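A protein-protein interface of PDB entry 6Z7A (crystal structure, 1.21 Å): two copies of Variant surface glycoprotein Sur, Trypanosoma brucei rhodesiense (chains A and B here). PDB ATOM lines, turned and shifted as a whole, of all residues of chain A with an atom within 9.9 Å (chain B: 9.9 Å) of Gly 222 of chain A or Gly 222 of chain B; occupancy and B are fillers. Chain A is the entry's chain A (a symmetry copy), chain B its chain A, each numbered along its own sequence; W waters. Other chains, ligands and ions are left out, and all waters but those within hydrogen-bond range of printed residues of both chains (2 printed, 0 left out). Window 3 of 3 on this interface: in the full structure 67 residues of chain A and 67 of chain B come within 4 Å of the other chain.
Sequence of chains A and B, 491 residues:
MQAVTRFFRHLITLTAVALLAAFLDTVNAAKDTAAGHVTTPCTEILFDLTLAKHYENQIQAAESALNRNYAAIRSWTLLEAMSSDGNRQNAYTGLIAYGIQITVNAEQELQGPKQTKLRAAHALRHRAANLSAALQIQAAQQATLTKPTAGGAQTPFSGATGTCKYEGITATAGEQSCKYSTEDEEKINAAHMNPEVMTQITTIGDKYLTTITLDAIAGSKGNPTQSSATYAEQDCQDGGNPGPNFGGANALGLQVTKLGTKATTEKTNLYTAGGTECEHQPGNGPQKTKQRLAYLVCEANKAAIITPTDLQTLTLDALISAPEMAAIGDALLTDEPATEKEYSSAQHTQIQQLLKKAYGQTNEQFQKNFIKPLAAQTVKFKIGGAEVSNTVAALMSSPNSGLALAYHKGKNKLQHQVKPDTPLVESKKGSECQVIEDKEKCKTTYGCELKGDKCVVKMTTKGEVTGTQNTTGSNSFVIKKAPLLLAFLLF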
ATOM      1  N   GLY A 159       1.974 -19.824  12.216  1.00  0.00           N
ATOM      2  CA  GLY A 159       1.974 -21.083  12.931  1.00  0.00           C
ATOM      3  C   GLY A 159       1.372 -21.069  14.314  1.00  0.00           C
ATOM      4  O   GLY A 159       1.381 -22.112  14.978  1.00  0.00           O
ATOM      5  N   ALA A 160       0.828 -19.929  14.773  1.00  0.00           N
ATOM      6  CA  ALA A 160       0.229 -19.861  16.094  1.00  0.00           C
ATOM      7  C   ALA A 160      -1.166 -20.488  16.084  1.00  0.00           C
ATOM      8  O   ALA A 160      -1.832 -20.554  15.042  1.00  0.00           O
ATOM      9  CB  ALA A 160       0.122 -18.385  16.527  1.00  0.00           C
ATOM     10  N   THR A 161      -1.593 -20.956  17.270  1.00  0.00           N
ATOM     11  CA  THR A 161      -2.986 -21.342  17.518  1.00  0.00           C
ATOM     12  C   THR A 161      -3.756 -20.261  18.238  1.00  0.00           C
ATOM     13  O   THR A 161      -4.989 -20.193  18.122  1.00  0.00           O
ATOM     14  CB  THR A 161      -3.081 -22.684  18.282  1.00  0.00           C
ATOM     15  OG1 THR A 161      -2.198 -22.747  19.410  1.00  0.00           O
ATOM     16  CG2 THR A 161      -2.778 -23.790  17.303  1.00  0.00           C
ATOM     17  N   GLY A 162      -3.023 -19.335  18.866  1.00  0.00           N
ATOM     18  CA  GLY A 162      -3.596 -18.155  19.497  1.00  0.00           C
ATOM     19  C   GLY A 162      -2.802 -16.923  19.182  1.00  0.00           C
ATOM     20  O   GLY A 162      -1.574 -16.938  19.232  1.00  0.00           O
ATOM     21  N   GLY A 219       2.898 -13.159  27.347  1.00  0.00           N
ATOM     22  CA  GLY A 219       2.566 -14.150  28.321  1.00  0.00           C
ATOM     23  C   GLY A 219       1.461 -15.040  27.827  1.00  0.00           C
ATOM     24  O   GLY A 219       0.548 -14.569  27.149  1.00  0.00           O
ATOM     25  N   SER A 220       1.535 -16.338  28.169  1.00  0.00           N
ATOM     26  CA  SER A 220       0.561 -17.351  27.720  1.00  0.00           C
ATOM     27  C   SER A 220       0.241 -18.283  28.866  1.00  0.00           C
ATOM     28  O   SER A 220       1.091 -18.548  29.722  1.00  0.00           O
ATOM     29  CB  SER A 220       1.174 -18.129  26.560  1.00  0.00           C
ATOM     30  OG  SER A 220       0.252 -18.993  25.849  1.00  0.00           O
ATOM     31  N   LYS A 221      -1.010 -18.747  28.863  1.00  0.00           N
ATOM     32  CA  LYS A 221      -1.462 -19.789  29.764  1.00  0.00           C
ATOM     33  C   LYS A 221      -2.467 -20.629  29.009  1.00  0.00           C
ATOM     34  O   LYS A 221      -3.296 -20.115  28.265  1.00  0.00           O
ATOM     35  CB  LYS A 221      -2.084 -19.166  31.011  1.00  0.00           C
ATOM     36  CG  LYS A 221      -2.779 -20.188  31.985  1.00  0.00           C
ATOM     37  CD  LYS A 221      -3.550 -19.402  33.032  1.00  0.00           C
ATOM     38  CE  LYS A 221      -4.391 -20.370  33.941  1.00  0.00           C
ATOM     39  NZ  LYS A 221      -5.110 -19.538  34.974  1.00  0.00           N
ATOM     40  N   GLY A 222      -2.416 -21.935  29.243  1.00  0.00           N
ATOM     41  CA  GLY A 222      -3.415 -22.751  28.591  1.00  0.00           C
ATOM     42  C   GLY A 222      -3.320 -22.777  27.078  1.00  0.00           C
ATOM     43  O   GLY A 222      -2.239 -22.881  26.496  1.00  0.00           O
ATOM     44  N   ASN A 223      -4.504 -22.761  26.439  1.00  0.00           N
ATOM     45  CA  ASN A 223      -4.672 -22.903  24.999  1.00  0.00           C
ATOM     46  C   ASN A 223      -5.443 -21.687  24.483  1.00  0.00           C
ATOM     47  O   ASN A 223      -6.623 -21.783  24.154  1.00  0.00           O
ATOM     48  CB  ASN A 223      -5.479 -24.181  24.735  1.00  0.00           C
ATOM     49  CG  ASN A 223      -5.767 -24.378  23.245  1.00  0.00           C
ATOM     50  OD1 ASN A 223      -4.961 -24.033  22.377  1.00  0.00           O
ATOM     51  ND2 ASN A 223      -6.856 -25.081  22.970  1.00  0.00           N
ATOM     52  N   PRO A 224      -4.805 -20.504  24.432  1.00  0.00           N
ATOM     53  CA  PRO A 224      -5.465 -19.329  23.840  1.00  0.00           C
ATOM     54  C   PRO A 224      -5.757 -19.531  22.357  1.00  0.00           C
ATOM     55  O   PRO A 224      -4.904 -20.011  21.603  1.00  0.00           O
ATOM     56  CB  PRO A 224      -4.412 -18.199  24.032  1.00  0.00           C
ATOM     57  CG  PRO A 224      -3.078 -18.907  24.117  1.00  0.00           C
ATOM     58  CD  PRO A 224      -3.412 -20.222  24.849  1.00  0.00           C
ATOM     59  N   THR A 225      -6.935 -19.069  21.922  1.00  0.00           N
ATOM     60  CA  THR A 225      -7.347 -19.203  20.523  1.00  0.00           C
ATOM     61  C   THR A 225      -8.187 -17.992  20.167  1.00  0.00           C
ATOM     62  O   THR A 225      -8.244 -17.003  20.918  1.00  0.00           O
ATOM     63  CB  THR A 225      -8.165 -20.497  20.289  1.00  0.00           C
ATOM     64  OG1 THR A 225      -9.423 -20.324  20.953  1.00  0.00           O
ATOM     65  CG2 THR A 225      -7.400 -21.703  20.788  1.00  0.00           C
ATOM     66  N   SER A 228     -10.621 -16.671  22.824  1.00  0.00           N
ATOM     67  CA  SER A 228     -10.173 -16.037  24.067  1.00  0.00           C
ATOM     68  C   SER A 228     -10.512 -14.543  23.999  1.00  0.00           C
ATOM     69  O   SER A 228      -9.646 -13.668  23.957  1.00  0.00           O
ATOM     70  CB  SER A 228      -8.655 -16.222  24.206  1.00  0.00           C
ATOM     71  OG  SER A 228      -8.363 -17.631  24.191  1.00  0.00           O
ATOM     72  N   CYS A 236      -6.206 -11.367  26.123  1.00  0.00           N
ATOM     73  CA  CYS A 236      -7.187 -12.266  25.529  1.00  0.00           C
ATOM     74  C   CYS A 236      -7.391 -13.501  26.411  1.00  0.00           C
ATOM     75  O   CYS A 236      -6.463 -14.285  26.569  1.00  0.00           O
ATOM     76  CB  CYS A 236      -6.660 -12.711  24.169  1.00  0.00           C
ATOM     77  SG  CYS A 236      -6.484 -11.382  22.946  1.00  0.00           S
ATOM     78  N   GLN A 237      -8.583 -13.650  26.996  1.00  0.00           N
ATOM     79  CA  GLN A 237      -8.873 -14.768  27.917  1.00  0.00           C
ATOM     80  C   GLN A 237     -10.166 -15.478  27.557  1.00  0.00           C
ATOM     81  O   GLN A 237     -11.104 -14.861  27.055  1.00  0.00           O
ATOM     82  CB  GLN A 237      -8.994 -14.287  29.331  1.00  0.00           C
ATOM     83  CG  GLN A 237      -7.609 -13.803  29.938  1.00  0.00           C
ATOM     84  CD  GLN A 237      -7.698 -13.535  31.431  1.00  0.00           C
ATOM     85  OE1 GLN A 237      -8.323 -14.304  32.181  1.00  0.00           O
ATOM     86  NE2 GLN A 237      -7.075 -12.426  31.881  1.00  0.00           N
ATOM     87  N   ASP A 238     -10.184 -16.793  27.824  1.00  0.00           N
ATOM     88  CA  ASP A 238     -11.450 -17.526  27.934  1.00  0.00           C
ATOM     89  C   ASP A 238     -11.252 -18.769  28.758  1.00  0.00           C
ATOM     90  O   ASP A 238     -10.128 -19.171  29.079  1.00  0.00           O
ATOM     91  CB  ASP A 238     -12.116 -17.839  26.594  1.00  0.00           C
ATOM     92  CG  ASP A 238     -11.448 -18.927  25.804  1.00  0.00           C
ATOM     93  OD1 ASP A 238     -10.222 -19.051  25.762  1.00  0.00           O
ATOM     94  OD2 ASP A 238     -12.219 -19.695  25.199  1.00  0.00           O
ATOM     95  N   GLY A 239     -12.392 -19.365  29.123  1.00  0.00           N
ATOM     96  CA  GLY A 239     -12.364 -20.570  29.925  1.00  0.00           C
ATOM     97  C   GLY A 239     -12.317 -20.265  31.404  1.00  0.00           C
ATOM     98  O   GLY A 239     -11.725 -19.278  31.857  1.00  0.00           O
ATOM     99  N   PHE A 246      -4.267 -13.404  34.533  1.00  0.00           N
ATOM    100  CA  PHE A 246      -4.621 -14.602  33.744  1.00  0.00           C
ATOM    101  C   PHE A 246      -5.523 -15.550  34.544  1.00  0.00           C
ATOM    102  O   PHE A 246      -5.259 -16.736  34.659  1.00  0.00           O
ATOM    103  CB  PHE A 246      -3.360 -15.343  33.262  1.00  0.00           C
ATOM    104  CG  PHE A 246      -2.599 -14.639  32.098  1.00  0.00           C
ATOM    105  CD1 PHE A 246      -3.001 -13.422  31.556  1.00  0.00           C
ATOM    106  CD2 PHE A 246      -1.509 -15.290  31.526  1.00  0.00           C
ATOM    107  CE1 PHE A 246      -2.291 -12.881  30.483  1.00  0.00           C
ATOM    108  CE2 PHE A 246      -0.836 -14.801  30.483  1.00  0.00           C
ATOM    109  CZ  PHE A 246      -1.226 -13.569  29.946  1.00  0.00           C
ATOM    110  N   GLY A 247      -6.558 -14.996  35.139  1.00  0.00           N
ATOM    111  CA  GLY A 247      -7.491 -15.835  35.893  1.00  0.00           C
ATOM    112  C   GLY A 247      -8.125 -16.953  35.071  1.00  0.00           C
ATOM    113  O   GLY A 247      -8.445 -18.038  35.595  1.00  0.00           O
ATOM    114  N   GLY A 248      -8.379 -16.692  33.811  1.00  0.00           N
ATOM    115  CA  GLY A 248      -9.042 -17.642  32.948  1.00  0.00           C
ATOM    116  C   GLY A 248      -8.185 -18.854  32.658  1.00  0.00           C
ATOM    117  O   GLY A 248      -6.985 -18.919  32.938  1.00  0.00           O
ATOM    118  N   ALA A 249      -8.848 -19.881  32.125  1.00  0.00           N
ATOM    119  CA  ALA A 249      -8.131 -21.104  31.776  1.00  0.00           C
ATOM    120  C   ALA A 249      -7.086 -20.852  30.672  1.00  0.00           C
ATOM    121  O   ALA A 249      -5.987 -21.435  30.689  1.00  0.00           O
ATOM    122  CB  ALA A 249      -9.144 -22.135  31.319  1.00  0.00           C
ATOM    123  N   ASN A 250      -7.453 -20.058  29.671  1.00  0.00           N
ATOM    124  CA  ASN A 250      -6.612 -19.800  28.500  1.00  0.00           C
ATOM    125  C   ASN A 250      -6.407 -18.301  28.422  1.00  0.00           C
ATOM    126  O   ASN A 250      -7.367 -17.516  28.516  1.00  0.00           O
ATOM    127  CB  ASN A 250      -7.318 -20.239  27.209  1.00  0.00           C
ATOM    128  CG  ASN A 250      -7.883 -21.634  27.315  1.00  0.00           C
ATOM    129  OD1 ASN A 250      -7.139 -22.569  27.582  1.00  0.00           O
ATOM    130  ND2 ASN A 250      -9.207 -21.775  27.147  1.00  0.00           N
ATOM    131  N   ALA A 251      -5.148 -17.908  28.242  1.00  0.00           N
ATOM    132  CA  ALA A 251      -4.807 -16.483  28.221  1.00  0.00           C
ATOM    133  C   ALA A 251      -3.606 -16.229  27.329  1.00  0.00           C
ATOM    134  O   ALA A 251      -2.664 -17.011  27.252  1.00  0.00           O
ATOM    135  CB  ALA A 251      -4.502 -15.953  29.631  1.00  0.00           C
ATOM    136  N   LEU A 252      -3.642 -15.060  26.705  1.00  0.00           N
ATOM    137  CA  LEU A 252      -2.510 -14.571  25.918  1.00  0.00           C
ATOM    138  C   LEU A 252      -2.533 -13.057  25.943  1.00  0.00           C
ATOM    139  O   LEU A 252      -3.601 -12.456  25.821  1.00  0.00           O
ATOM    140  CB  LEU A 252      -2.642 -15.025  24.443  1.00  0.00           C
ATOM    141  CG  LEU A 252      -1.491 -14.675  23.464  1.00  0.00           C
ATOM    142  CD1 LEU A 252      -0.155 -15.143  23.922  1.00  0.00           C
ATOM    143  CD2 LEU A 252      -1.823 -15.229  22.097  1.00  0.00           C
ATOM    144  N   GLY B 159       0.357 -14.769  36.368  1.00  0.00           N
ATOM    145  CA  GLY B 159      -0.441 -15.949  36.110  1.00  0.00           C
ATOM    146  C   GLY B 159      -0.092 -16.737  34.872  1.00  0.00           C
ATOM    147  O   GLY B 159      -0.769 -17.733  34.590  1.00  0.00           O
ATOM    148  N   ALA B 160       0.954 -16.343  34.126  1.00  0.00           N
ATOM    149  CA  ALA B 160       1.337 -17.069  32.927  1.00  0.00           C
ATOM    150  C   ALA B 160       2.113 -18.336  33.293  1.00  0.00           C
ATOM    151  O   ALA B 160       2.727 -18.425  34.364  1.00  0.00           O
ATOM    152  CB  ALA B 160       2.224 -16.165  32.049  1.00  0.00           C
ATOM    153  N   THR B 161       2.063 -19.322  32.379  1.00  0.00           N
ATOM    154  CA  THR B 161       2.947 -20.491  32.422  1.00  0.00           C
ATOM    155  C   THR B 161       4.115 -20.357  31.475  1.00  0.00           C
ATOM    156  O   THR B 161       5.169 -20.974  31.694  1.00  0.00           O
ATOM    157  CB  THR B 161       2.173 -21.804  32.156  1.00  0.00           C
ATOM    158  OG1 THR B 161       1.298 -21.715  31.024  1.00  0.00           O
ATOM    159  CG2 THR B 161       1.398 -22.139  33.406  1.00  0.00           C
ATOM    160  N   GLY B 162       3.983 -19.448  30.503  1.00  0.00           N
ATOM    161  CA  GLY B 162       5.057 -19.097  29.585  1.00  0.00           C
ATOM    162  C   GLY B 162       5.152 -17.614  29.392  1.00  0.00           C
ATOM    163  O   GLY B 162       4.141 -16.937  29.217  1.00  0.00           O
ATOM    164  N   GLY B 219       1.801 -14.199  19.881  1.00  0.00           N
ATOM    165  CA  GLY B 219       1.399 -15.453  19.328  1.00  0.00           C
ATOM    166  C   GLY B 219       1.839 -16.593  20.202  1.00  0.00           C
ATOM    167  O   GLY B 219       2.923 -16.540  20.782  1.00  0.00           O
ATOM    168  N   SER B 220       0.999 -17.637  20.299  1.00  0.00           N
ATOM    169  CA  SER B 220       1.257 -18.808  21.158  1.00  0.00           C
ATOM    170  C   SER B 220       0.860 -20.068  20.422  1.00  0.00           C
ATOM    171  O   SER B 220      -0.074 -20.061  19.614  1.00  0.00           O
ATOM    172  CB  SER B 220       0.439 -18.661  22.436  1.00  0.00           C
ATOM    173  OG  SER B 220       0.769 -19.605  23.486  1.00  0.00           O
ATOM    174  N   LYS B 221       1.611 -21.133  20.711  1.00  0.00           N
ATOM    175  CA  LYS B 221       1.284 -22.469  20.257  1.00  0.00           C
ATOM    176  C   LYS B 221       1.700 -23.429  21.348  1.00  0.00           C
ATOM    177  O   LYS B 221       2.749 -23.274  21.967  1.00  0.00           O
ATOM    178  CB  LYS B 221       2.013 -22.768  18.949  1.00  0.00           C
ATOM    179  CG  LYS B 221       1.887 -24.253  18.444  1.00  0.00           C
ATOM    180  CD  LYS B 221       2.851 -24.448  17.287  1.00  0.00           C
ATOM    181  CE  LYS B 221       2.882 -25.955  16.841  1.00  0.00           C
ATOM    182  NZ  LYS B 221       3.833 -26.081  15.676  1.00  0.00           N
ATOM    183  N   GLY B 222       0.885 -24.457  21.552  1.00  0.00           N
ATOM    184  CA  GLY B 222       1.299 -25.428  22.539  1.00  0.00           C
ATOM    185  C   GLY B 222       1.370 -24.897  23.957  1.00  0.00           C
ATOM    186  O   GLY B 222       0.495 -24.164  24.421  1.00  0.00           O
ATOM    187  N   ASN B 223       2.409 -25.354  24.679  1.00  0.00           N
ATOM    188  CA  ASN B 223       2.619 -25.085  26.095  1.00  0.00           C
ATOM    189  C   ASN B 223       3.998 -24.443  26.262  1.00  0.00           C
ATOM    190  O   ASN B 223       4.936 -25.084  26.729  1.00  0.00           O
ATOM    191  CB  ASN B 223       2.570 -26.419  26.849  1.00  0.00           C
ATOM    192  CG  ASN B 223       2.851 -26.244  28.342  1.00  0.00           C
ATOM    193  OD1 ASN B 223       2.488 -25.238  28.958  1.00  0.00           O
ATOM    194  ND2 ASN B 223       3.363 -27.306  28.949  1.00  0.00           N
ATOM    195  N   PRO B 224       4.163 -23.173  25.854  1.00  0.00           N
ATOM    196  CA  PRO B 224       5.436 -22.474  26.095  1.00  0.00           C
ATOM    197  C   PRO B 224       5.717 -22.307  27.584  1.00  0.00           C
ATOM    198  O   PRO B 224       4.829 -21.931  28.358  1.00  0.00           O
ATOM    199  CB  PRO B 224       5.207 -21.085  25.431  1.00  0.00           C
ATOM    200  CG  PRO B 224       3.709 -20.881  25.441  1.00  0.00           C
ATOM    201  CD  PRO B 224       3.148 -22.300  25.221  1.00  0.00           C
ATOM    202  N   THR B 225       6.985 -22.493  27.968  1.00  0.00           N
ATOM    203  CA  THR B 225       7.394 -22.370  29.369  1.00  0.00           C
ATOM    204  C   THR B 225       8.808 -21.826  29.396  1.00  0.00           C
ATOM    205  O   THR B 225       9.341 -21.362  28.373  1.00  0.00           O
ATOM    206  CB  THR B 225       7.341 -23.734  30.101  1.00  0.00           C
ATOM    207  OG1 THR B 225       8.392 -24.543  29.556  1.00  0.00           O
ATOM    208  CG2 THR B 225       5.975 -24.365  29.946  1.00  0.00           C
ATOM    209  N   SER B 228      11.258 -23.100  26.730  1.00  0.00           N
ATOM    210  CA  SER B 228      11.123 -22.776  25.308  1.00  0.00           C
ATOM    211  C   SER B 228      12.262 -21.826  24.917  1.00  0.00           C
ATOM    212  O   SER B 228      12.065 -20.659  24.577  1.00  0.00           O
ATOM    213  CB  SER B 228       9.769 -22.090  25.074  1.00  0.00           C
ATOM    214  OG  SER B 228       8.726 -22.975  25.520  1.00  0.00           O
ATOM    215  N   CYS B 236      10.356 -17.670  21.419  1.00  0.00           N
ATOM    216  CA  CYS B 236      10.702 -18.712  22.377  1.00  0.00           C
ATOM    217  C   CYS B 236      10.064 -20.046  21.977  1.00  0.00           C
ATOM    218  O   CYS B 236       8.845 -20.155  21.986  1.00  0.00           O
ATOM    219  CB  CYS B 236      10.165 -18.298  23.743  1.00  0.00           C
ATOM    220  SG  CYS B 236      10.914 -16.798  24.436  1.00  0.00           S
ATOM    221  N   GLN B 237      10.885 -21.033  21.605  1.00  0.00           N
ATOM    222  CA  GLN B 237      10.381 -22.340  21.139  1.00  0.00           C
ATOM    223  C   GLN B 237      11.063 -23.497  21.848  1.00  0.00           C
ATOM    224  O   GLN B 237      12.233 -23.407  22.218  1.00  0.00           O
ATOM    225  CB  GLN B 237      10.603 -22.513  19.666  1.00  0.00           C
ATOM    226  CG  GLN B 237       9.690 -21.555  18.790  1.00  0.00           C
ATOM    227  CD  GLN B 237       9.755 -21.894  17.309  1.00  0.00           C
ATOM    228  OE1 GLN B 237       9.742 -23.076  16.925  1.00  0.00           O
ATOM    229  NE2 GLN B 237       9.837 -20.852  16.456  1.00  0.00           N
ATOM    230  N   ASP B 238      10.296 -24.582  22.030  1.00  0.00           N
ATOM    231  CA  ASP B 238      10.892 -25.894  22.304  1.00  0.00           C
ATOM    232  C   ASP B 238       9.930 -26.984  21.917  1.00  0.00           C
ATOM    233  O   ASP B 238       8.752 -26.747  21.627  1.00  0.00           O
ATOM    234  CB  ASP B 238      11.397 -26.071  23.736  1.00  0.00           C
ATOM    235  CG  ASP B 238      10.316 -26.246  24.762  1.00  0.00           C
ATOM    236  OD1 ASP B 238       9.254 -25.623  24.711  1.00  0.00           O
ATOM    237  OD2 ASP B 238      10.567 -27.067  25.665  1.00  0.00           O
ATOM    238  N   GLY B 239      10.476 -28.205  21.893  1.00  0.00           N
ATOM    239  CA  GLY B 239       9.676 -29.357  21.533  1.00  0.00           C
ATOM    240  C   GLY B 239       9.654 -29.587  20.039  1.00  0.00           C
ATOM    241  O   GLY B 239       9.690 -28.655  19.227  1.00  0.00           O
ATOM    242  N   PHE B 246       6.710 -20.847  13.986  1.00  0.00           N
ATOM    243  CA  PHE B 246       6.396 -21.691  15.158  1.00  0.00           C
ATOM    244  C   PHE B 246       6.499 -23.182  14.815  1.00  0.00           C
ATOM    245  O   PHE B 246       5.593 -23.959  15.068  1.00  0.00           O
ATOM    246  CB  PHE B 246       4.998 -21.366  15.719  1.00  0.00           C
ATOM    247  CG  PHE B 246       4.908 -20.020  16.498  1.00  0.00           C
ATOM    248  CD1 PHE B 246       5.991 -19.159  16.650  1.00  0.00           C
ATOM    249  CD2 PHE B 246       3.712 -19.696  17.132  1.00  0.00           C
ATOM    250  CE1 PHE B 246       5.839 -17.993  17.404  1.00  0.00           C
ATOM    251  CE2 PHE B 246       3.557 -18.602  17.878  1.00  0.00           C
ATOM    252  CZ  PHE B 246       4.637 -17.723  18.019  1.00  0.00           C
ATOM    253  N   GLY B 247       7.594 -23.555  14.186  1.00  0.00           N
ATOM    254  CA  GLY B 247       7.790 -24.967  13.854  1.00  0.00           C
ATOM    255  C   GLY B 247       7.753 -25.900  15.061  1.00  0.00           C
ATOM    256  O   GLY B 247       7.335 -27.070  14.959  1.00  0.00           O
ATOM    257  N   GLY B 248       8.243 -25.436  16.185  1.00  0.00           N
ATOM    258  CA  GLY B 248       8.331 -26.246  17.377  1.00  0.00           C
ATOM    259  C   GLY B 248       6.971 -26.570  17.955  1.00  0.00           C
ATOM    260  O   GLY B 248       5.929 -26.024  17.585  1.00  0.00           O
ATOM    261  N   ALA B 249       6.978 -27.547  18.865  1.00  0.00           N
ATOM    262  CA  ALA B 249       5.732 -27.939  19.516  1.00  0.00           C
ATOM    263  C   ALA B 249       5.146 -26.789  20.357  1.00  0.00           C
ATOM    264  O   ALA B 249       3.917 -26.603  20.415  1.00  0.00           O
ATOM    265  CB  ALA B 249       6.013 -29.144  20.392  1.00  0.00           C
ATOM    266  N   ASN B 250       6.007 -26.075  21.075  1.00  0.00           N
ATOM    267  CA  ASN B 250       5.597 -25.014  21.999  1.00  0.00           C
ATOM    268  C   ASN B 250       6.298 -23.746  21.559  1.00  0.00           C
ATOM    269  O   ASN B 250       7.518 -23.737  21.316  1.00  0.00           O
ATOM    270  CB  ASN B 250       6.058 -25.325  23.431  1.00  0.00           C
ATOM    271  CG  ASN B 250       5.706 -26.732  23.849  1.00  0.00           C
ATOM    272  OD1 ASN B 250       4.537 -27.095  23.826  1.00  0.00           O
ATOM    273  ND2 ASN B 250       6.719 -27.541  24.196  1.00  0.00           N
ATOM    274  N   ALA B 251       5.520 -22.670  21.463  1.00  0.00           N
ATOM    275  CA  ALA B 251       6.062 -21.398  20.979  1.00  0.00           C
ATOM    276  C   ALA B 251       5.328 -20.226  21.604  1.00  0.00           C
ATOM    277  O   ALA B 251       4.122 -20.248  21.831  1.00  0.00           O
ATOM    278  CB  ALA B 251       5.967 -21.288  19.449  1.00  0.00           C
ATOM    279  N   LEU B 252       6.094 -19.164  21.810  1.00  0.00           N
ATOM    280  CA  LEU B 252       5.539 -17.890  22.266  1.00  0.00           C
ATOM    281  C   LEU B 252       6.423 -16.775  21.749  1.00  0.00           C
ATOM    282  O   LEU B 252       7.648 -16.895  21.780  1.00  0.00           O
ATOM    283  CB  LEU B 252       5.544 -17.822  23.814  1.00  0.00           C
ATOM    284  CG  LEU B 252       4.915 -16.579  24.494  1.00  0.00           C
ATOM    285  CD1 LEU B 252       3.512 -16.315  24.074  1.00  0.00           C
ATOM    286  CD2 LEU B 252       5.014 -16.737  25.994  1.00  0.00           C
HETATM  287  O   HOH W   1      -0.752 -23.571  30.811  1.00  0.00           O
HETATM  288  O   HOH W   2      -1.572 -25.246  20.438  1.00  0.00           O
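The backbone NH (N) of Thr 161 of chain B sits at hydrogen-bond distance from the backbone carbonyl oxygen (O) of Ser 220 of chain A (2.9 Å). The backbone NH (N) of Ser 220 of chain A lies within hydrogen-bond range of the backbone carbonyl oxygen (O) of Gly 162 of chain B, at 2.9 Å. O of Ser 220 of chain B sits at hydrogen-bond distance from N of Thr 161 of chain A, at 2.9 Å. O of Gly 162 of chain A lies within hydrogen-bond range of N of Ser 220 of chain B. The side-chain hydroxyl of Ser 220 of chain A sits at hydrogen-bond distance from the side-chain hydroxyl of Ser 220 of chain B.
N of Gly 162 of chain B lies close to O of Pro 224 of chain B, 3.4 Å away. The side-chain amino group (NZ) of Lys 221 of chain B lies within hydrogen-bond range of the backbone carbonyl oxygen (O) of Gly 248 of chain B (2.8 Å). The backbone carbonyl oxygen (O) of Lys 221 of chain B lies within hydrogen-bond range of the backbone NH (N) of Ala 251 of chain B, at 2.9 Å. The backbone carbonyl oxygen (O) of Pro 224 of chain A lies close to the backbone NH (N) of Gly 162 of chain A (3.4 Å). The backbone carbonyl oxygen of Phe 246 of chain A sits at hydrogen-bond distance from the side-chain amino group of Lys 221 of chain A (2.8 Å).
CB of Ala 160 of chain A touches O of Ser 220 of chain B, 3.5 Å away. Lys 221 of chain B touches Thr 161 of chain A (CA to OG1, 3.6 Å). O of Gly 162 of chain A touches CA of Gly 219 of chain B, at 3.3 Å. CA of Gly 219 of chain A touches O of Gly 162 of chain B, 3.3 Å away. CB of Ser 220 of chain A touches CD1 of Leu 252 of chain B, at 3.9 Å. OG1 of Thr 161 of chain B touches CA of Lys 221 of chain A, at 3.6 Å. Gly 159 of chain B touches Phe 246 of chain A. Phe 246 of chain A touches Ala 160 of chain B (CD2 to CA, 3.6 Å). CD1 of Leu 252 of chain A touches CB of Ser 220 of chain B, at 3.9 Å. CD1 of Leu 252 of chain A touches CD1 of Leu 252 of chain B, at 3.9 Å.
Of the printed residues of chain B, Gly 159 of chain A touches Lys 221 and Phe 246. Gly 222 of chain A touches just one residue of chain B: Gly 222. Gln 237 of chain A touches none of the printed residues of chain B. Printed residues of chain A within 4 Å of Gly 219 of chain B: Gly 162 (3.3 Å). Printed residues of chain A within 4 Å of Ser 220 of chain B: Ala 160 (3.5 Å), Thr 161 (2.9 Å), Gly 162 (2.9 Å), Ser 220 (2.5 Å), Pro 224 (3.9 Å) and Leu 252 (3.9 Å). Gly 222 of chain B touches one residue of chain A. The nearest residue of chain B that does not touch Gly 222 of chain A is Thr 161 of chain B (4.1 Å).
Printed residues of chain B that touch a printed residue of chain A: Gly 159, Ala 160, Thr 161, Gly 162, Gly 219, Ser 220, Lys 221, Gly 222, Pro 224, Phe 246 and Leu 252. Among the printed residues, no Asp or Glu carboxylate lies within 4 Å of a Lys or Arg side-chain nitrogen of the other chain.
Gly 159 of chain A touches Lys 221 of chain B, and with the chains exchanged Lys 221 of chain A touches Gly 159 of chain B. Ala 160 of chain A touches Ser 220 of chain B, and with the chains exchanged Ser 220 of chain A touches Ala 160 of chain B. Ala 160 of chain A touches Phe 246 of chain B, and with the chains exchanged Phe 246 of chain A touches Ala 160 of chain B. Gly 162 of chain A touches Gly 219 of chain B, and with the chains exchanged Gly 219 of chain A touches Gly 162 of chain B.
Water W1 lies within hydrogen-bond range of the side-chain hydroxyl of Thr 161 of chain B (2.8 Å) and the backbone NH of Gly 222 of chain A (2.8 Å). Water W2 bridges OG1 of Thr 161 of chain A (2.8 Å) and N of Gly 222 of chain B (2.8 Å).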
